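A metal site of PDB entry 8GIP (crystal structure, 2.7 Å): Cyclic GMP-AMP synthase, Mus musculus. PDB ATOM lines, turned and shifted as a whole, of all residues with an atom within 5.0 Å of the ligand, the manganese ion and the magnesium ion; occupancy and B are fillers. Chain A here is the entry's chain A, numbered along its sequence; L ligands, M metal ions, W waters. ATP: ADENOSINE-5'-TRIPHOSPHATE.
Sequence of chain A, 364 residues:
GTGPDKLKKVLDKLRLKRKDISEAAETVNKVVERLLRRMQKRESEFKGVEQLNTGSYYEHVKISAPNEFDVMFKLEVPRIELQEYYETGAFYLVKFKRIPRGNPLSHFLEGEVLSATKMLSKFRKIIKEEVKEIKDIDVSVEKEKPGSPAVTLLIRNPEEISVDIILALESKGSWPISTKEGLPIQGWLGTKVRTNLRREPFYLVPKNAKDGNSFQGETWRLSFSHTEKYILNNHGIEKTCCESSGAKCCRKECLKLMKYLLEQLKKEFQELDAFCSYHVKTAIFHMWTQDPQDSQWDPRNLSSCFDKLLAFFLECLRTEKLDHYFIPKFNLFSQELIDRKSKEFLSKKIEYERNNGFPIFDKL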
ATOM      1  N   GLY A  55      15.446 -15.987 -23.204  1.00  0.00           N
ATOM      2  CA  GLY A  55      14.055 -15.724 -22.915  1.00  0.00           C
ATOM      3  C   GLY A  55      13.539 -14.463 -23.557  1.00  0.00           C
ATOM      4  O   GLY A  55      14.213 -13.796 -24.343  1.00  0.00           O
ATOM      5  N   SER A  56      12.297 -14.123 -23.208  1.00  0.00           N
ATOM      6  CA  SER A  56      11.575 -13.178 -24.037  1.00  0.00           C
ATOM      7  C   SER A  56      12.214 -11.808 -23.971  1.00  0.00           C
ATOM      8  O   SER A  56      12.384 -11.152 -25.008  1.00  0.00           O
ATOM      9  CB  SER A  56      10.096 -13.121 -23.657  1.00  0.00           C
ATOM     10  OG  SER A  56       9.895 -12.790 -22.289  1.00  0.00           O
ATOM     11  N   GLU A  59      14.866 -11.541 -26.405  1.00  0.00           N
ATOM     12  CA  GLU A  59      14.394 -11.741 -27.765  1.00  0.00           C
ATOM     13  C   GLU A  59      13.517 -10.587 -28.242  1.00  0.00           C
ATOM     14  O   GLU A  59      13.190 -10.529 -29.435  1.00  0.00           O
ATOM     15  CB  GLU A  59      13.616 -13.041 -27.839  1.00  0.00           C
ATOM     16  CG  GLU A  59      14.426 -14.271 -27.488  1.00  0.00           C
ATOM     17  CD  GLU A  59      13.553 -15.482 -27.104  1.00  0.00           C
ATOM     18  OE1 GLU A  59      12.350 -15.296 -26.755  1.00  0.00           O
ATOM     19  OE2 GLU A  59      14.076 -16.623 -27.144  1.00  0.00           O
ATOM     20  N   LYS A  62       9.031  -9.912 -24.784  1.00  0.00           N
ATOM     21  CA  LYS A  62       8.461  -9.714 -23.463  1.00  0.00           C
ATOM     22  C   LYS A  62       7.365  -8.669 -23.533  1.00  0.00           C
ATOM     23  O   LYS A  62       7.605  -7.562 -24.024  1.00  0.00           O
ATOM     24  CB  LYS A  62       9.563  -9.284 -22.481  1.00  0.00           C
ATOM     25  CG  LYS A  62       9.167  -9.067 -21.032  1.00  0.00           C
ATOM     26  CD  LYS A  62       8.541 -10.281 -20.409  1.00  0.00           C
ATOM     27  CE  LYS A  62       8.040  -9.942 -19.043  1.00  0.00           C
ATOM     28  NZ  LYS A  62       6.662 -10.415 -18.728  1.00  0.00           N
ATOM     29  N   GLU A  68      10.037 -10.060 -15.852  1.00  0.00           N
ATOM     30  CA  GLU A  68      10.542 -11.427 -15.764  1.00  0.00           C
ATOM     31  C   GLU A  68      11.714 -11.586 -16.709  1.00  0.00           C
ATOM     32  O   GLU A  68      11.572 -11.412 -17.922  1.00  0.00           O
ATOM     33  CB  GLU A  68       9.437 -12.425 -16.073  1.00  0.00           C
ATOM     34  CG  GLU A  68       9.674 -13.749 -15.444  1.00  0.00           C
ATOM     35  CD  GLU A  68      10.423 -14.675 -16.357  1.00  0.00           C
ATOM     36  OE1 GLU A  68      10.637 -14.309 -17.541  1.00  0.00           O
ATOM     37  OE2 GLU A  68      10.821 -15.761 -15.911  1.00  0.00           O
ATOM     38  N   ASP A  70      15.276 -14.035 -17.773  1.00  0.00           N
ATOM     39  CA  ASP A  70      15.824 -15.386 -17.718  1.00  0.00           C
ATOM     40  C   ASP A  70      17.325 -15.347 -17.976  1.00  0.00           C
ATOM     41  O   ASP A  70      17.763 -14.710 -18.944  1.00  0.00           O
ATOM     42  CB  ASP A  70      15.137 -16.301 -18.717  1.00  0.00           C
ATOM     43  CG  ASP A  70      13.639 -16.345 -18.510  1.00  0.00           C
ATOM     44  OD1 ASP A  70      13.194 -17.023 -17.576  1.00  0.00           O
ATOM     45  OD2 ASP A  70      12.899 -15.702 -19.275  1.00  0.00           O
ATOM     46  N   ASP A 164      14.917 -15.692 -13.258  1.00  0.00           N
ATOM     47  CA  ASP A 164      15.214 -17.113 -13.204  1.00  0.00           C
ATOM     48  C   ASP A 164      16.703 -17.286 -13.464  1.00  0.00           C
ATOM     49  O   ASP A 164      17.172 -17.050 -14.588  1.00  0.00           O
ATOM     50  CB  ASP A 164      14.380 -17.869 -14.231  1.00  0.00           C
ATOM     51  CG  ASP A 164      12.952 -18.064 -13.780  1.00  0.00           C
ATOM     52  OD1 ASP A 164      12.682 -17.896 -12.568  1.00  0.00           O
ATOM     53  OD2 ASP A 164      12.098 -18.400 -14.612  1.00  0.00           O
ATOM     54  N   ARG A 221      17.393 -32.298 -18.603  1.00  0.00           N
ATOM     55  CA  ARG A 221      16.585 -31.984 -19.767  1.00  0.00           C
ATOM     56  C   ARG A 221      17.393 -31.094 -20.706  1.00  0.00           C
ATOM     57  O   ARG A 221      18.110 -30.195 -20.244  1.00  0.00           O
ATOM     58  CB  ARG A 221      15.271 -31.291 -19.331  1.00  0.00           C
ATOM     59  CG  ARG A 221      14.304 -30.920 -20.467  1.00  0.00           C
ATOM     60  CD  ARG A 221      13.424 -29.734 -20.091  1.00  0.00           C
ATOM     61  NE  ARG A 221      13.885 -28.516 -20.754  1.00  0.00           N
ATOM     62  CZ  ARG A 221      13.891 -27.314 -20.184  1.00  0.00           C
ATOM     63  NH1 ARG A 221      13.349 -27.109 -18.986  1.00  0.00           N
ATOM     64  NH2 ARG A 221      14.481 -26.293 -20.823  1.00  0.00           N
ATOM     65  N   PHE A 224      17.607 -25.380 -25.496  1.00  0.00           N
ATOM     66  CA  PHE A 224      18.003 -24.715 -26.734  1.00  0.00           C
ATOM     67  C   PHE A 224      17.642 -23.239 -26.702  1.00  0.00           C
ATOM     68  O   PHE A 224      17.414 -22.649 -27.753  1.00  0.00           O
ATOM     69  CB  PHE A 224      17.375 -25.406 -27.956  1.00  0.00           C
ATOM     70  CG  PHE A 224      17.919 -26.796 -28.186  1.00  0.00           C
ATOM     71  CD1 PHE A 224      19.184 -26.977 -28.730  1.00  0.00           C
ATOM     72  CD2 PHE A 224      17.195 -27.907 -27.783  1.00  0.00           C
ATOM     73  CE1 PHE A 224      19.703 -28.240 -28.918  1.00  0.00           C
ATOM     74  CE2 PHE A 224      17.709 -29.186 -27.952  1.00  0.00           C
ATOM     75  CZ  PHE A 224      18.968 -29.360 -28.519  1.00  0.00           C
ATOM     76  N   SER A 225      17.595 -22.640 -25.500  1.00  0.00           N
ATOM     77  CA  SER A 225      17.239 -21.229 -25.410  1.00  0.00           C
ATOM     78  C   SER A 225      18.198 -20.370 -26.191  1.00  0.00           C
ATOM     79  O   SER A 225      17.816 -19.296 -26.658  1.00  0.00           O
ATOM     80  CB  SER A 225      17.215 -20.729 -23.977  1.00  0.00           C
ATOM     81  OG  SER A 225      16.408 -21.549 -23.178  1.00  0.00           O
ATOM     82  N   GLU A 228      17.099 -20.599 -29.813  1.00  0.00           N
ATOM     83  CA  GLU A 228      15.816 -19.908 -29.977  1.00  0.00           C
ATOM     84  C   GLU A 228      16.021 -18.387 -29.976  1.00  0.00           C
ATOM     85  O   GLU A 228      15.363 -17.667 -30.743  1.00  0.00           O
ATOM     86  CB  GLU A 228      14.865 -20.340 -28.861  1.00  0.00           C
ATOM     87  CG  GLU A 228      14.655 -21.852 -28.761  1.00  0.00           C
ATOM     88  CD  GLU A 228      13.998 -22.231 -27.449  1.00  0.00           C
ATOM     89  OE1 GLU A 228      13.689 -21.300 -26.662  1.00  0.00           O
ATOM     90  OE2 GLU A 228      13.768 -23.437 -27.195  1.00  0.00           O
ATOM     91  N   LYS A 259       1.136 -14.811 -27.109  1.00  0.00           N
ATOM     92  CA  LYS A 259       1.635 -14.891 -25.734  1.00  0.00           C
ATOM     93  C   LYS A 259       0.635 -14.260 -24.778  1.00  0.00           C
ATOM     94  O   LYS A 259       0.437 -14.753 -23.655  1.00  0.00           O
ATOM     95  CB  LYS A 259       2.978 -14.180 -25.612  1.00  0.00           C
ATOM     96  CG  LYS A 259       4.150 -14.987 -25.998  1.00  0.00           C
ATOM     97  CD  LYS A 259       5.377 -14.087 -26.135  1.00  0.00           C
ATOM     98  CE  LYS A 259       5.766 -13.473 -24.804  1.00  0.00           C
ATOM     99  NZ  LYS A 259       6.396 -14.517 -23.951  1.00  0.00           N
ATOM    100  N   GLU A 263      -1.477 -15.576 -21.526  1.00  0.00           N
ATOM    101  CA  GLU A 263      -1.342 -14.954 -20.206  1.00  0.00           C
ATOM    102  C   GLU A 263      -2.690 -14.516 -19.648  1.00  0.00           C
ATOM    103  O   GLU A 263      -3.035 -14.822 -18.500  1.00  0.00           O
ATOM    104  CB  GLU A 263      -0.403 -13.743 -20.263  1.00  0.00           C
ATOM    105  CG  GLU A 263       1.059 -14.088 -20.421  1.00  0.00           C
ATOM    106  CD  GLU A 263       2.008 -12.902 -20.246  1.00  0.00           C
ATOM    107  OE1 GLU A 263       1.614 -11.877 -19.650  1.00  0.00           O
ATOM    108  OE2 GLU A 263       3.190 -13.005 -20.691  1.00  0.00           O
ATOM    109  N   CYS A 276       1.959 -23.235 -20.817  1.00  0.00           N
ATOM    110  CA  CYS A 276       2.938 -22.199 -20.569  1.00  0.00           C
ATOM    111  C   CYS A 276       3.230 -21.527 -21.902  1.00  0.00           C
ATOM    112  O   CYS A 276       2.767 -21.967 -22.952  1.00  0.00           O
ATOM    113  CB  CYS A 276       4.207 -22.761 -19.925  1.00  0.00           C
ATOM    114  SG  CYS A 276       5.138 -23.903 -20.944  1.00  0.00           S
ATOM    115  N   SER A 277       4.015 -20.462 -21.842  1.00  0.00           N
ATOM    116  CA  SER A 277       4.258 -19.679 -23.030  1.00  0.00           C
ATOM    117  C   SER A 277       5.102 -20.437 -24.034  1.00  0.00           C
ATOM    118  O   SER A 277       4.996 -20.187 -25.241  1.00  0.00           O
ATOM    119  CB  SER A 277       4.911 -18.349 -22.663  1.00  0.00           C
ATOM    120  OG  SER A 277       6.191 -18.558 -22.108  1.00  0.00           O
ATOM    121  N   TYR A 278       5.945 -21.361 -23.560  1.00  0.00           N
ATOM    122  CA  TYR A 278       6.785 -22.141 -24.455  1.00  0.00           C
ATOM    123  C   TYR A 278       5.947 -22.965 -25.414  1.00  0.00           C
ATOM    124  O   TYR A 278       6.396 -23.335 -26.506  1.00  0.00           O
ATOM    125  CB  TYR A 278       7.714 -23.058 -23.644  1.00  0.00           C
ATOM    126  CG  TYR A 278       8.802 -23.662 -24.496  1.00  0.00           C
ATOM    127  CD1 TYR A 278       9.791 -22.855 -25.028  1.00  0.00           C
ATOM    128  CD2 TYR A 278       8.822 -25.012 -24.801  1.00  0.00           C
ATOM    129  CE1 TYR A 278      10.803 -23.377 -25.834  1.00  0.00           C
ATOM    130  CE2 TYR A 278       9.817 -25.554 -25.622  1.00  0.00           C
ATOM    131  CZ  TYR A 278      10.813 -24.718 -26.125  1.00  0.00           C
ATOM    132  OH  TYR A 278      11.836 -25.185 -26.916  1.00  0.00           O
ATOM    133  N   LYS A 281       5.376 -20.500 -28.018  1.00  0.00           N
ATOM    134  CA  LYS A 281       6.643 -20.236 -28.700  1.00  0.00           C
ATOM    135  C   LYS A 281       6.974 -21.367 -29.666  1.00  0.00           C
ATOM    136  O   LYS A 281       7.470 -21.127 -30.773  1.00  0.00           O
ATOM    137  CB  LYS A 281       7.778 -20.041 -27.699  1.00  0.00           C
ATOM    138  CG  LYS A 281       9.110 -19.581 -28.275  1.00  0.00           C
ATOM    139  CD  LYS A 281      10.127 -19.388 -27.151  1.00  0.00           C
ATOM    140  CE  LYS A 281      11.347 -18.614 -27.604  1.00  0.00           C
ATOM    141  NZ  LYS A 281      12.573 -18.859 -26.760  1.00  0.00           N
ATOM    142  N   HIS A 324       8.163 -30.928 -29.994  1.00  0.00           N
ATOM    143  CA  HIS A 324       9.303 -30.073 -29.695  1.00  0.00           C
ATOM    144  C   HIS A 324       9.983 -29.679 -31.000  1.00  0.00           C
ATOM    145  O   HIS A 324      10.189 -30.517 -31.894  1.00  0.00           O
ATOM    146  CB  HIS A 324      10.282 -30.810 -28.779  1.00  0.00           C
ATOM    147  CG  HIS A 324      11.214 -29.907 -28.023  1.00  0.00           C
ATOM    148  ND1 HIS A 324      12.190 -29.150 -28.629  1.00  0.00           N
ATOM    149  CD2 HIS A 324      11.335 -29.686 -26.697  1.00  0.00           C
ATOM    150  CE1 HIS A 324      12.865 -28.470 -27.713  1.00  0.00           C
ATOM    151  NE2 HIS A 324      12.367 -28.776 -26.525  1.00  0.00           N
HETATM  152  PG  ATP L   1       7.721 -15.212 -20.876  1.00  0.00           P
HETATM  153  O1G ATP L   1       6.508 -16.055 -20.681  1.00  0.00           O
HETATM  154  O2G ATP L   1       7.496 -13.753 -21.303  1.00  0.00           O
HETATM  155  O3G ATP L   1       8.643 -15.170 -19.643  1.00  0.00           O
HETATM  156  PB  ATP L   1       9.843 -16.864 -22.176  1.00  0.00           P
HETATM  157  O1B ATP L   1       9.944 -17.519 -23.483  1.00  0.00           O
HETATM  158  O2B ATP L   1      11.074 -16.110 -21.663  1.00  0.00           O
HETATM  159  O3B ATP L   1       8.629 -15.847 -22.022  1.00  0.00           O
HETATM  160  PA  ATP L   1      10.016 -18.524 -19.784  1.00  0.00           P
HETATM  161  O1A ATP L   1       8.963 -19.335 -19.130  1.00  0.00           O
HETATM  162  O2A ATP L   1      10.569 -17.288 -19.085  1.00  0.00           O
HETATM  163  O3A ATP L   1       9.451 -17.984 -21.121  1.00  0.00           O
HETATM  164  O5' ATP L   1      11.190 -19.513 -20.166  1.00  0.00           O
HETATM  165  C5' ATP L   1      12.510 -19.028 -20.488  1.00  0.00           C
HETATM  166  C4' ATP L   1      13.082 -19.851 -21.623  1.00  0.00           C
HETATM  167  O4' ATP L   1      13.414 -21.185 -21.154  1.00  0.00           O
HETATM  168  C3' ATP L   1      12.180 -20.074 -22.825  1.00  0.00           C
HETATM  169  O3' ATP L   1      12.264 -19.010 -23.765  1.00  0.00           O
HETATM  170  C2' ATP L   1      12.738 -21.372 -23.409  1.00  0.00           C
HETATM  171  O2' ATP L   1      13.914 -21.140 -24.179  1.00  0.00           O
HETATM  172  C1' ATP L   1      13.091 -22.157 -22.143  1.00  0.00           C
HETATM  173  N9  ATP L   1      11.962 -22.957 -21.677  1.00  0.00           N
HETATM  174  C8  ATP L   1      10.895 -22.546 -20.910  1.00  0.00           C
HETATM  175  N7  ATP L   1       9.998 -23.468 -20.698  1.00  0.00           N
HETATM  176  C5  ATP L   1      10.492 -24.568 -21.397  1.00  0.00           C
HETATM  177  C6  ATP L   1      10.007 -25.880 -21.568  1.00  0.00           C
HETATM  178  N6  ATP L   1       8.870 -26.333 -21.019  1.00  0.00           N
HETATM  179  N1  ATP L   1      10.739 -26.727 -22.320  1.00  0.00           N
HETATM  180  C2  ATP L   1      11.871 -26.283 -22.867  1.00  0.00           C
HETATM  181  N3  ATP L   1      12.435 -25.077 -22.779  1.00  0.00           N
HETATM  182  C4  ATP L   1      11.694 -24.266 -22.011  1.00  0.00           C
HETATM  183 MN    MN M   1      11.029 -17.808 -16.670  1.00  0.00          MN
HETATM  184 MG    MG M   2      10.721 -15.268 -19.504  1.00  0.00          MG
HETATM  185  O   HOH W   1      11.351 -13.513 -20.059  1.00  0.00           O
HETATM  186  O   HOH W   2      14.770 -24.718 -24.697  1.00  0.00           O
HETATM  187  O   HOH W   3       5.949 -11.684 -21.429  1.00  0.00           O
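OE1 of Glu 228 is in salt-bridge range of NZ of Lys 281 (2.7 Å).
OE2 of Glu 59 is in salt-bridge range of NZ of Lys 281 (2.7 Å).
The side-chain carboxylate of Glu 228 sits at hydrogen-bond distance from the side-chain hydroxyl of Tyr 278, at 2.6 Å.
N of Tyr 278 sits close to SG of Cys 276, at 3.7 Å.
Of the 18 residues printed, 3 come within 4 Å of the manganese ion.
The nearest printed residue that does not touch the manganese ion is Gly 55 (7.2 Å).
Gly 55 touches the ligand.
CD of Lys 62 touches O2G of the ligand, at 3.7 Å.
Tyr 278 touches the ligand.
Of the 18 residues printed, 12 come within 4 Å of the ligand.
Water W1 lies within hydrogen-bond range of OG of Ser 56 (2.8 Å) and O of Glu 68 (3.0 Å).
Water W3 lies within hydrogen-bond range of O2G of the ligand, NZ of Lys 62 and OE2 of Glu 263.
Water W2 lies within hydrogen-bond range of the side-chain carboxylate of Glu 228, the backbone NH of Phe 224 and a nitrogen (N3) of the ligand.
The magnesium ion is bound by water W1 (1.9 Å), an oxygen (O2A) of the ligand (2.1 Å), an oxygen (O3G) of the ligand (2.1 Å), the side-chain carboxylate of Glu 68 (2.2 Å), the side-chain carboxylate of Asp 70 (2.2 Å) and an oxygen (O2B) of the ligand (2.3 Å).
An oxygen (O2') of the ligand sits at hydrogen-bond distance from the side-chain hydroxyl of Ser 225, 2.7 Å away.
The side-chain amino group (NZ) of Lys 259 is in salt-bridge range of an oxygen (O2G) of the ligand, 3.0 Å away.
An oxygen (O2G) of the ligand sits at hydrogen-bond distance from the side-chain hydroxyl of Ser 56 (2.8 Å).
O1G of the ligand sits at hydrogen-bond distance from OG of Ser 277, 2.9 Å away.
NZ of Lys 281 sits at hydrogen-bond distance from O3' of the ligand (3.0 Å).
The backbone NH (N) of Ser 56 lies close to an oxygen (O2B) of the ligand (2.8 Å).
A nitrogen (N3) of the ligand lies within hydrogen-bond range of the guanidinium group (NH2) of Arg 221, 3.1 Å away.
OE1 of Glu 228 lies within hydrogen-bond range of O2' of the ligand (2.5 Å).
The manganese ion is bound by OE2 of Glu 68 (2.2 Å), OD2 of Asp 164 (2.4 Å), OD1 of Asp 70 (2.5 Å) and O2A of the ligand (2.5 Å).
OG of Ser 56 touches the magnesium ion, 3.8 Å away.
Three residues have an atom within 4 Å of the magnesium ion: Ser 56, Glu 68 and Asp 70.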
